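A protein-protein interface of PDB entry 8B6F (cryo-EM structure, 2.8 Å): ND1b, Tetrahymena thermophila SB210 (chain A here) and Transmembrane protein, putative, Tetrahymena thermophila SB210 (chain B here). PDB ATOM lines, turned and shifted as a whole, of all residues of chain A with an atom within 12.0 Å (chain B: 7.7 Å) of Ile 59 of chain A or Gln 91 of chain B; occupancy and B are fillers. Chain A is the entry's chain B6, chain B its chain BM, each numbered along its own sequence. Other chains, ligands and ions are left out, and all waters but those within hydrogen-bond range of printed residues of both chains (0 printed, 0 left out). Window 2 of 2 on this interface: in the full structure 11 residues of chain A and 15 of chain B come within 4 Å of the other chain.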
ATOM      1  N   PHE A  50     -32.432 -14.938  14.494  1.00  0.00           N
ATOM      2  CA  PHE A  50     -32.883 -16.325  14.511  1.00  0.00           C
ATOM      3  C   PHE A  50     -32.917 -16.902  13.101  1.00  0.00           C
ATOM      4  O   PHE A  50     -32.521 -18.053  12.885  1.00  0.00           O
ATOM      5  CB  PHE A  50     -34.262 -16.423  15.164  1.00  0.00           C
ATOM      6  CG  PHE A  50     -34.216 -16.717  16.636  1.00  0.00           C
ATOM      7  CD1 PHE A  50     -34.135 -15.691  17.562  1.00  0.00           C
ATOM      8  CD2 PHE A  50     -34.262 -18.024  17.095  1.00  0.00           C
ATOM      9  CE1 PHE A  50     -34.095 -15.961  18.917  1.00  0.00           C
ATOM     10  CE2 PHE A  50     -34.223 -18.300  18.447  1.00  0.00           C
ATOM     11  CZ  PHE A  50     -34.140 -17.267  19.360  1.00  0.00           C
ATOM     12  N   ASN A  51     -33.388 -16.120  12.129  1.00  0.00           N
ATOM     13  CA  ASN A  51     -33.387 -16.592  10.748  1.00  0.00           C
ATOM     14  C   ASN A  51     -31.968 -16.837  10.260  1.00  0.00           C
ATOM     15  O   ASN A  51     -31.701 -17.838   9.586  1.00  0.00           O
ATOM     16  CB  ASN A  51     -34.095 -15.585   9.843  1.00  0.00           C
ATOM     17  CG  ASN A  51     -35.600 -15.727   9.877  1.00  0.00           C
ATOM     18  OD1 ASN A  51     -36.133 -16.695  10.417  1.00  0.00           O
ATOM     19  ND2 ASN A  51     -36.296 -14.766   9.282  1.00  0.00           N
ATOM     20  N   LEU A  52     -31.043 -15.932  10.585  1.00  0.00           N
ATOM     21  CA  LEU A  52     -29.651 -16.136  10.197  1.00  0.00           C
ATOM     22  C   LEU A  52     -29.101 -17.414  10.812  1.00  0.00           C
ATOM     23  O   LEU A  52     -28.417 -18.193  10.139  1.00  0.00           O
ATOM     24  CB  LEU A  52     -28.807 -14.936  10.626  1.00  0.00           C
ATOM     25  CG  LEU A  52     -29.062 -13.618   9.895  1.00  0.00           C
ATOM     26  CD1 LEU A  52     -28.499 -12.452  10.679  1.00  0.00           C
ATOM     27  CD2 LEU A  52     -28.417 -13.663   8.542  1.00  0.00           C
ATOM     28  N   CYS A  53     -29.382 -17.640  12.095  1.00  0.00           N
ATOM     29  CA  CYS A  53     -28.893 -18.843  12.758  1.00  0.00           C
ATOM     30  C   CYS A  53     -29.474 -20.104  12.129  1.00  0.00           C
ATOM     31  O   CYS A  53     -28.754 -21.086  11.913  1.00  0.00           O
ATOM     32  CB  CYS A  53     -29.233 -18.778  14.246  1.00  0.00           C
ATOM     33  SG  CYS A  53     -28.272 -17.564  15.169  1.00  0.00           S
ATOM     34  N   PHE A  54     -30.776 -20.100  11.830  1.00  0.00           N
ATOM     35  CA  PHE A  54     -31.393 -21.275  11.221  1.00  0.00           C
ATOM     36  C   PHE A  54     -30.840 -21.541   9.826  1.00  0.00           C
ATOM     37  O   PHE A  54     -30.595 -22.696   9.462  1.00  0.00           O
ATOM     38  CB  PHE A  54     -32.911 -21.106  11.170  1.00  0.00           C
ATOM     39  CG  PHE A  54     -33.574 -21.128  12.522  1.00  0.00           C
ATOM     40  CD1 PHE A  54     -33.105 -21.950  13.534  1.00  0.00           C
ATOM     41  CD2 PHE A  54     -34.670 -20.324  12.776  1.00  0.00           C
ATOM     42  CE1 PHE A  54     -33.715 -21.968  14.770  1.00  0.00           C
ATOM     43  CE2 PHE A  54     -35.286 -20.339  14.011  1.00  0.00           C
ATOM     44  CZ  PHE A  54     -34.808 -21.162  15.009  1.00  0.00           C
ATOM     45  N   VAL A  55     -30.634 -20.490   9.033  1.00  0.00           N
ATOM     46  CA  VAL A  55     -30.080 -20.674   7.694  1.00  0.00           C
ATOM     47  C   VAL A  55     -28.666 -21.224   7.781  1.00  0.00           C
ATOM     48  O   VAL A  55     -28.272 -22.097   7.000  1.00  0.00           O
ATOM     49  CB  VAL A  55     -30.135 -19.353   6.902  1.00  0.00           C
ATOM     50  CG1 VAL A  55     -29.252 -19.414   5.662  1.00  0.00           C
ATOM     51  CG2 VAL A  55     -31.562 -19.059   6.500  1.00  0.00           C
ATOM     52  N   THR A  56     -27.878 -20.720   8.728  1.00  0.00           N
ATOM     53  CA  THR A  56     -26.537 -21.254   8.924  1.00  0.00           C
ATOM     54  C   THR A  56     -26.592 -22.720   9.333  1.00  0.00           C
ATOM     55  O   THR A  56     -25.778 -23.531   8.878  1.00  0.00           O
ATOM     56  CB  THR A  56     -25.800 -20.426   9.973  1.00  0.00           C
ATOM     57  OG1 THR A  56     -25.782 -19.049   9.577  1.00  0.00           O
ATOM     58  CG2 THR A  56     -24.381 -20.896  10.096  1.00  0.00           C
ATOM     59  N   PHE A  57     -27.538 -23.075  10.204  1.00  0.00           N
ATOM     60  CA  PHE A  57     -27.673 -24.463  10.634  1.00  0.00           C
ATOM     61  C   PHE A  57     -28.017 -25.375   9.464  1.00  0.00           C
ATOM     62  O   PHE A  57     -27.446 -26.463   9.328  1.00  0.00           O
ATOM     63  CB  PHE A  57     -28.744 -24.557  11.724  1.00  0.00           C
ATOM     64  CG  PHE A  57     -29.133 -25.964  12.083  1.00  0.00           C
ATOM     65  CD1 PHE A  57     -30.133 -26.621  11.384  1.00  0.00           C
ATOM     66  CD2 PHE A  57     -28.525 -26.616  13.142  1.00  0.00           C
ATOM     67  CE1 PHE A  57     -30.500 -27.907  11.717  1.00  0.00           C
ATOM     68  CE2 PHE A  57     -28.889 -27.904  13.480  1.00  0.00           C
ATOM     69  CZ  PHE A  57     -29.878 -28.550  12.766  1.00  0.00           C
ATOM     70  N   PHE A  58     -28.951 -24.955   8.611  1.00  0.00           N
ATOM     71  CA  PHE A  58     -29.397 -25.811   7.518  1.00  0.00           C
ATOM     72  C   PHE A  58     -28.390 -25.869   6.379  1.00  0.00           C
ATOM     73  O   PHE A  58     -28.254 -26.914   5.736  1.00  0.00           O
ATOM     74  CB  PHE A  58     -30.755 -25.335   6.998  1.00  0.00           C
ATOM     75  CG  PHE A  58     -31.908 -25.732   7.872  1.00  0.00           C
ATOM     76  CD1 PHE A  58     -32.327 -27.051   7.930  1.00  0.00           C
ATOM     77  CD2 PHE A  58     -32.573 -24.789   8.636  1.00  0.00           C
ATOM     78  CE1 PHE A  58     -33.386 -27.421   8.733  1.00  0.00           C
ATOM     79  CE2 PHE A  58     -33.633 -25.152   9.444  1.00  0.00           C
ATOM     80  CZ  PHE A  58     -34.040 -26.470   9.492  1.00  0.00           C
ATOM     81  N   ILE A  59     -27.686 -24.775   6.105  1.00  0.00           N
ATOM     82  CA  ILE A  59     -26.695 -24.768   5.038  1.00  0.00           C
ATOM     83  C   ILE A  59     -25.438 -25.481   5.521  1.00  0.00           C
ATOM     84  O   ILE A  59     -24.574 -24.876   6.155  1.00  0.00           O
ATOM     85  CB  ILE A  59     -26.375 -23.333   4.571  1.00  0.00           C
ATOM     86  CG1 ILE A  59     -27.611 -22.706   3.925  1.00  0.00           C
ATOM     87  CG2 ILE A  59     -25.205 -23.333   3.589  1.00  0.00           C
ATOM     88  CD1 ILE A  59     -27.440 -21.251   3.528  1.00  0.00           C
ATOM     89  N   ASP B  77     -23.619 -27.077  16.997  1.00  0.00           N
ATOM     90  CA  ASP B  77     -23.995 -27.962  15.902  1.00  0.00           C
ATOM     91  C   ASP B  77     -22.962 -27.920  14.785  1.00  0.00           C
ATOM     92  O   ASP B  77     -22.619 -28.955  14.206  1.00  0.00           O
ATOM     93  CB  ASP B  77     -25.371 -27.578  15.365  1.00  0.00           C
ATOM     94  CG  ASP B  77     -25.737 -28.347  14.116  1.00  0.00           C
ATOM     95  OD1 ASP B  77     -26.052 -29.549  14.227  1.00  0.00           O
ATOM     96  OD2 ASP B  77     -25.702 -27.749  13.020  1.00  0.00           O
ATOM     97  N   ALA B  78     -22.453 -26.728  14.475  1.00  0.00           N
ATOM     98  CA  ALA B  78     -21.443 -26.603  13.432  1.00  0.00           C
ATOM     99  C   ALA B  78     -20.174 -27.362  13.784  1.00  0.00           C
ATOM    100  O   ALA B  78     -19.585 -28.035  12.929  1.00  0.00           O
ATOM    101  CB  ALA B  78     -21.120 -25.131  13.216  1.00  0.00           C
ATOM    102  N   ARG B  81     -20.801 -31.027  13.319  1.00  0.00           N
ATOM    103  CA  ARG B  81     -21.011 -31.496  11.953  1.00  0.00           C
ATOM    104  C   ARG B  81     -19.750 -32.055  11.311  1.00  0.00           C
ATOM    105  O   ARG B  81     -19.803 -32.451  10.142  1.00  0.00           O
ATOM    106  CB  ARG B  81     -21.558 -30.364  11.083  1.00  0.00           C
ATOM    107  CG  ARG B  81     -23.051 -30.145  11.224  1.00  0.00           C
ATOM    108  CD  ARG B  81     -23.529 -29.006  10.346  1.00  0.00           C
ATOM    109  NE  ARG B  81     -23.527 -29.365   8.934  1.00  0.00           N
ATOM    110  CZ  ARG B  81     -23.932 -28.566   7.956  1.00  0.00           C
ATOM    111  NH1 ARG B  81     -24.375 -27.344   8.201  1.00  0.00           N
ATOM    112  NH2 ARG B  81     -23.889 -29.003   6.702  1.00  0.00           N
ATOM    113  N   GLN B  86     -17.023 -34.269   3.691  1.00  0.00           N
ATOM    114  CA  GLN B  86     -16.468 -32.935   3.473  1.00  0.00           C
ATOM    115  C   GLN B  86     -17.487 -31.959   2.905  1.00  0.00           C
ATOM    116  O   GLN B  86     -17.612 -30.848   3.449  1.00  0.00           O
ATOM    117  CB  GLN B  86     -15.241 -33.037   2.561  1.00  0.00           C
ATOM    118  CG  GLN B  86     -14.609 -31.694   2.216  1.00  0.00           C
ATOM    119  CD  GLN B  86     -14.196 -30.910   3.443  1.00  0.00           C
ATOM    120  OE1 GLN B  86     -13.991 -31.474   4.516  1.00  0.00           O
ATOM    121  NE2 GLN B  86     -14.075 -29.597   3.291  1.00  0.00           N
ATOM    122  N   PRO B  87     -18.233 -32.280   1.845  1.00  0.00           N
ATOM    123  CA  PRO B  87     -19.160 -31.280   1.288  1.00  0.00           C
ATOM    124  C   PRO B  87     -20.264 -30.867   2.242  1.00  0.00           C
ATOM    125  O   PRO B  87     -20.862 -29.804   2.040  1.00  0.00           O
ATOM    126  CB  PRO B  87     -19.726 -31.977   0.043  1.00  0.00           C
ATOM    127  CG  PRO B  87     -19.506 -33.425   0.273  1.00  0.00           C
ATOM    128  CD  PRO B  87     -18.245 -33.530   1.067  1.00  0.00           C
ATOM    129  N   TYR B  88     -20.556 -31.663   3.270  1.00  0.00           N
ATOM    130  CA  TYR B  88     -21.665 -31.387   4.174  1.00  0.00           C
ATOM    131  C   TYR B  88     -21.206 -30.899   5.542  1.00  0.00           C
ATOM    132  O   TYR B  88     -22.028 -30.789   6.456  1.00  0.00           O
ATOM    133  CB  TYR B  88     -22.535 -32.634   4.319  1.00  0.00           C
ATOM    134  CG  TYR B  88     -22.917 -33.216   2.983  1.00  0.00           C
ATOM    135  CD1 TYR B  88     -23.810 -32.555   2.153  1.00  0.00           C
ATOM    136  CD2 TYR B  88     -22.367 -34.409   2.541  1.00  0.00           C
ATOM    137  CE1 TYR B  88     -24.157 -33.072   0.925  1.00  0.00           C
ATOM    138  CE2 TYR B  88     -22.707 -34.936   1.312  1.00  0.00           C
ATOM    139  CZ  TYR B  88     -23.599 -34.259   0.508  1.00  0.00           C
ATOM    140  OH  TYR B  88     -23.948 -34.771  -0.719  1.00  0.00           O
ATOM    141  N   LYS B  89     -19.920 -30.605   5.706  1.00  0.00           N
ATOM    142  CA  LYS B  89     -19.465 -29.991   6.940  1.00  0.00           C
ATOM    143  C   LYS B  89     -19.962 -28.551   7.015  1.00  0.00           C
ATOM    144  O   LYS B  89     -20.341 -27.940   6.013  1.00  0.00           O
ATOM    145  CB  LYS B  89     -17.940 -30.026   7.031  1.00  0.00           C
ATOM    146  CG  LYS B  89     -17.356 -31.428   7.060  1.00  0.00           C
ATOM    147  CD  LYS B  89     -15.851 -31.394   7.259  1.00  0.00           C
ATOM    148  CE  LYS B  89     -15.264 -32.792   7.294  1.00  0.00           C
ATOM    149  NZ  LYS B  89     -15.801 -33.597   8.422  1.00  0.00           N
ATOM    150  N   SER B  90     -19.962 -28.008   8.228  1.00  0.00           N
ATOM    151  CA  SER B  90     -20.519 -26.682   8.449  1.00  0.00           C
ATOM    152  C   SER B  90     -19.805 -25.639   7.604  1.00  0.00           C
ATOM    153  O   SER B  90     -18.573 -25.577   7.578  1.00  0.00           O
ATOM    154  CB  SER B  90     -20.436 -26.283   9.915  1.00  0.00           C
ATOM    155  OG  SER B  90     -21.025 -25.001  10.058  1.00  0.00           O
ATOM    156  N   GLN B  91     -20.587 -24.813   6.909  1.00  0.00           N
ATOM    157  CA  GLN B  91     -20.005 -23.733   6.126  1.00  0.00           C
ATOM    158  C   GLN B  91     -19.426 -22.635   7.010  1.00  0.00           C
ATOM    159  O   GLN B  91     -18.660 -21.802   6.516  1.00  0.00           O
ATOM    160  CB  GLN B  91     -21.048 -23.144   5.178  1.00  0.00           C
ATOM    161  CG  GLN B  91     -20.480 -22.104   4.227  1.00  0.00           C
ATOM    162  CD  GLN B  91     -21.456 -21.715   3.140  1.00  0.00           C
ATOM    163  OE1 GLN B  91     -22.483 -22.361   2.951  1.00  0.00           O
ATOM    164  NE2 GLN B  91     -21.139 -20.649   2.415  1.00  0.00           N
ATOM    165  N   ILE B  92     -19.772 -22.613   8.299  1.00  0.00           N
ATOM    166  CA  ILE B  92     -19.123 -21.684   9.222  1.00  0.00           C
ATOM    167  C   ILE B  92     -17.630 -21.971   9.280  1.00  0.00           C
ATOM    168  O   ILE B  92     -16.799 -21.056   9.229  1.00  0.00           O
ATOM    169  CB  ILE B  92     -19.745 -21.778  10.629  1.00  0.00           C
ATOM    170  CG1 ILE B  92     -21.261 -21.578  10.601  1.00  0.00           C
ATOM    171  CG2 ILE B  92     -19.095 -20.755  11.559  1.00  0.00           C
ATOM    172  CD1 ILE B  92     -21.902 -21.864  11.949  1.00  0.00           C
ATOM    173  N   LEU B  93     -17.269 -23.246   9.394  1.00  0.00           N
ATOM    174  CA  LEU B  93     -15.876 -23.650   9.507  1.00  0.00           C
ATOM    175  C   LEU B  93     -15.209 -23.858   8.157  1.00  0.00           C
ATOM    176  O   LEU B  93     -13.998 -23.641   8.037  1.00  0.00           O
ATOM    177  CB  LEU B  93     -15.774 -24.939  10.328  1.00  0.00           C
ATOM    178  CG  LEU B  93     -16.526 -24.940  11.662  1.00  0.00           C
ATOM    179  CD1 LEU B  93     -16.292 -26.244  12.404  1.00  0.00           C
ATOM    180  CD2 LEU B  93     -16.120 -23.757  12.523  1.00  0.00           C
ATOM    181  N   HIS B  94     -15.961 -24.271   7.142  1.00  0.00           N
ATOM    182  CA  HIS B  94     -15.423 -24.532   5.815  1.00  0.00           C
ATOM    183  C   HIS B  94     -15.978 -23.509   4.834  1.00  0.00           C
ATOM    184  O   HIS B  94     -17.178 -23.220   4.844  1.00  0.00           O
ATOM    185  CB  HIS B  94     -15.767 -25.950   5.362  1.00  0.00           C
ATOM    186  CG  HIS B  94     -15.211 -27.011   6.257  1.00  0.00           C
ATOM    187  ND1 HIS B  94     -14.005 -27.632   6.016  1.00  0.00           N
ATOM    188  CD2 HIS B  94     -15.688 -27.548   7.404  1.00  0.00           C
ATOM    189  CE1 HIS B  94     -13.768 -28.513   6.971  1.00  0.00           C
ATOM    190  NE2 HIS B  94     -14.774 -28.481   7.826  1.00  0.00           N
ATOM    191  N   GLY B  95     -15.101 -22.963   3.996  1.00  0.00           N
ATOM    192  CA  GLY B  95     -15.486 -21.914   3.069  1.00  0.00           C
ATOM    193  C   GLY B  95     -15.925 -22.467   1.723  1.00  0.00           C
ATOM    194  O   GLY B  95     -15.292 -23.360   1.165  1.00  0.00           O
ATOM    195  N   ARG B  96     -17.033 -21.921   1.216  1.00  0.00           N
ATOM    196  CA  ARG B  96     -17.562 -22.256  -0.109  1.00  0.00           C
ATOM    197  C   ARG B  96     -18.027 -20.945  -0.740  1.00  0.00           C
ATOM    198  O   ARG B  96     -19.173 -20.527  -0.553  1.00  0.00           O
ATOM    199  CB  ARG B  96     -18.693 -23.271  -0.017  1.00  0.00           C
ATOM    200  CG  ARG B  96     -18.334 -24.527   0.757  1.00  0.00           C
ATOM    201  CD  ARG B  96     -19.511 -25.485   0.824  1.00  0.00           C
ATOM    202  NE  ARG B  96     -19.185 -26.698   1.566  1.00  0.00           N
ATOM    203  CZ  ARG B  96     -19.303 -26.833   2.879  1.00  0.00           C
ATOM    204  NH1 ARG B  96     -19.731 -25.841   3.642  1.00  0.00           N
ATOM    205  NH2 ARG B  96     -18.984 -27.994   3.443  1.00  0.00           N
ATOM    206  N   GLN B  97     -17.139 -20.308  -1.489  1.00  0.00           N
ATOM    207  CA  GLN B  97     -17.370 -18.996  -2.067  1.00  0.00           C
ATOM    208  C   GLN B  97     -17.096 -19.030  -3.561  1.00  0.00           C
ATOM    209  O   GLN B  97     -16.393 -19.920  -4.051  1.00  0.00           O
ATOM    210  CB  GLN B  97     -16.488 -17.935  -1.390  1.00  0.00           C
ATOM    211  CG  GLN B  97     -16.860 -17.680   0.066  1.00  0.00           C
ATOM    212  CD  GLN B  97     -15.935 -16.692   0.749  1.00  0.00           C
ATOM    213  OE1 GLN B  97     -14.757 -16.595   0.413  1.00  0.00           O
ATOM    214  NE2 GLN B  97     -16.467 -15.951   1.713  1.00  0.00           N
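The backbone carbonyl oxygen (O) of Phe 57 of chain A lies within hydrogen-bond range of the guanidinium group (NH1) of Arg 81 of chain B, at 3.4 Å. O of Ile 59 of chain A is in hydrogen-bond range of NH1 of Arg 81 of chain B (3.2 Å).
NH2 of Arg 81 of chain B lies within hydrogen-bond range of O of Tyr 88 of chain B, at 2.6 Å. The side-chain hydroxyl of Ser 90 of chain B lies close to the backbone NH of Ile 92 of chain B. OG1 of Thr 56 of chain A is in hydrogen-bond range of O of Leu 52 of chain A, at 2.8 Å.
Thr 56 of chain A touches Ile 92 of chain B. OD2 of Asp 77 of chain B touches CD2 of Phe 57 of chain A, at 3.0 Å. CG2 of Ile 59 of chain A touches OE1 of Gln 91 of chain B (3.0 Å).
Of the printed residues of chain B, Ile 59 of chain A touches Arg 81 (3.2 Å) and Gln 91 (3.0 Å). Of chain A, only Ile 59 (3.0 Å) comes within 4 Å of Gln 91 of chain B. No residue of chain A comes within 4 Å of Ser 90 of chain B. Ile 92 of chain B touches just one residue of chain A: Thr 56. No residue of chain A comes within 4 Å of Leu 93 of chain B. No residue of chain A comes within 4 Å of His 94 of chain B. Gly 95 of chain B touches none of the printed residues of chain A. No residue of chain A comes within 4 Å of Arg 96 of chain B. Of the printed residues of chain B, Thr 56 of chain A touches Ile 92. Of the printed residues of chain B, Phe 57 of chain A touches Asp 77 (3.0 Å) and Arg 81 (3.4 Å). Of the printed residues of chain A, Arg 81 of chain B touches Phe 57 (3.4 Å) and Ile 59 (3.2 Å). Of the printed residues of chain A, Asp 77 of chain B touches Phe 57. Phe 50 of chain A touches none of the printed residues of chain B. Gln 97 of chain B touches none of the printed residues of chain A. The nearest residue of chain B that does not touch Ile 59 of chain A is Ser 90 of chain B (5.0 Å). The nearest printed residue of chain B that does not touch Phe 57 of chain A is Ile 92 of chain B (6.0 Å).
Of the 10 printed residues of chain A, 3 touch a printed residue of chain B. Printed residues of chain A that touch a printed residue of chain B: Thr 56, Phe 57 and Ile 59. Hydrophobic or aromatic side chains of chain A that line the printed part of chain B: Phe 57 and Ile 59. Hydrophobic or aromatic side chains of chain B within 4 Å of the printed part of chain A: Ile 92. Among the printed residues, 5 pairs touch across the chains.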
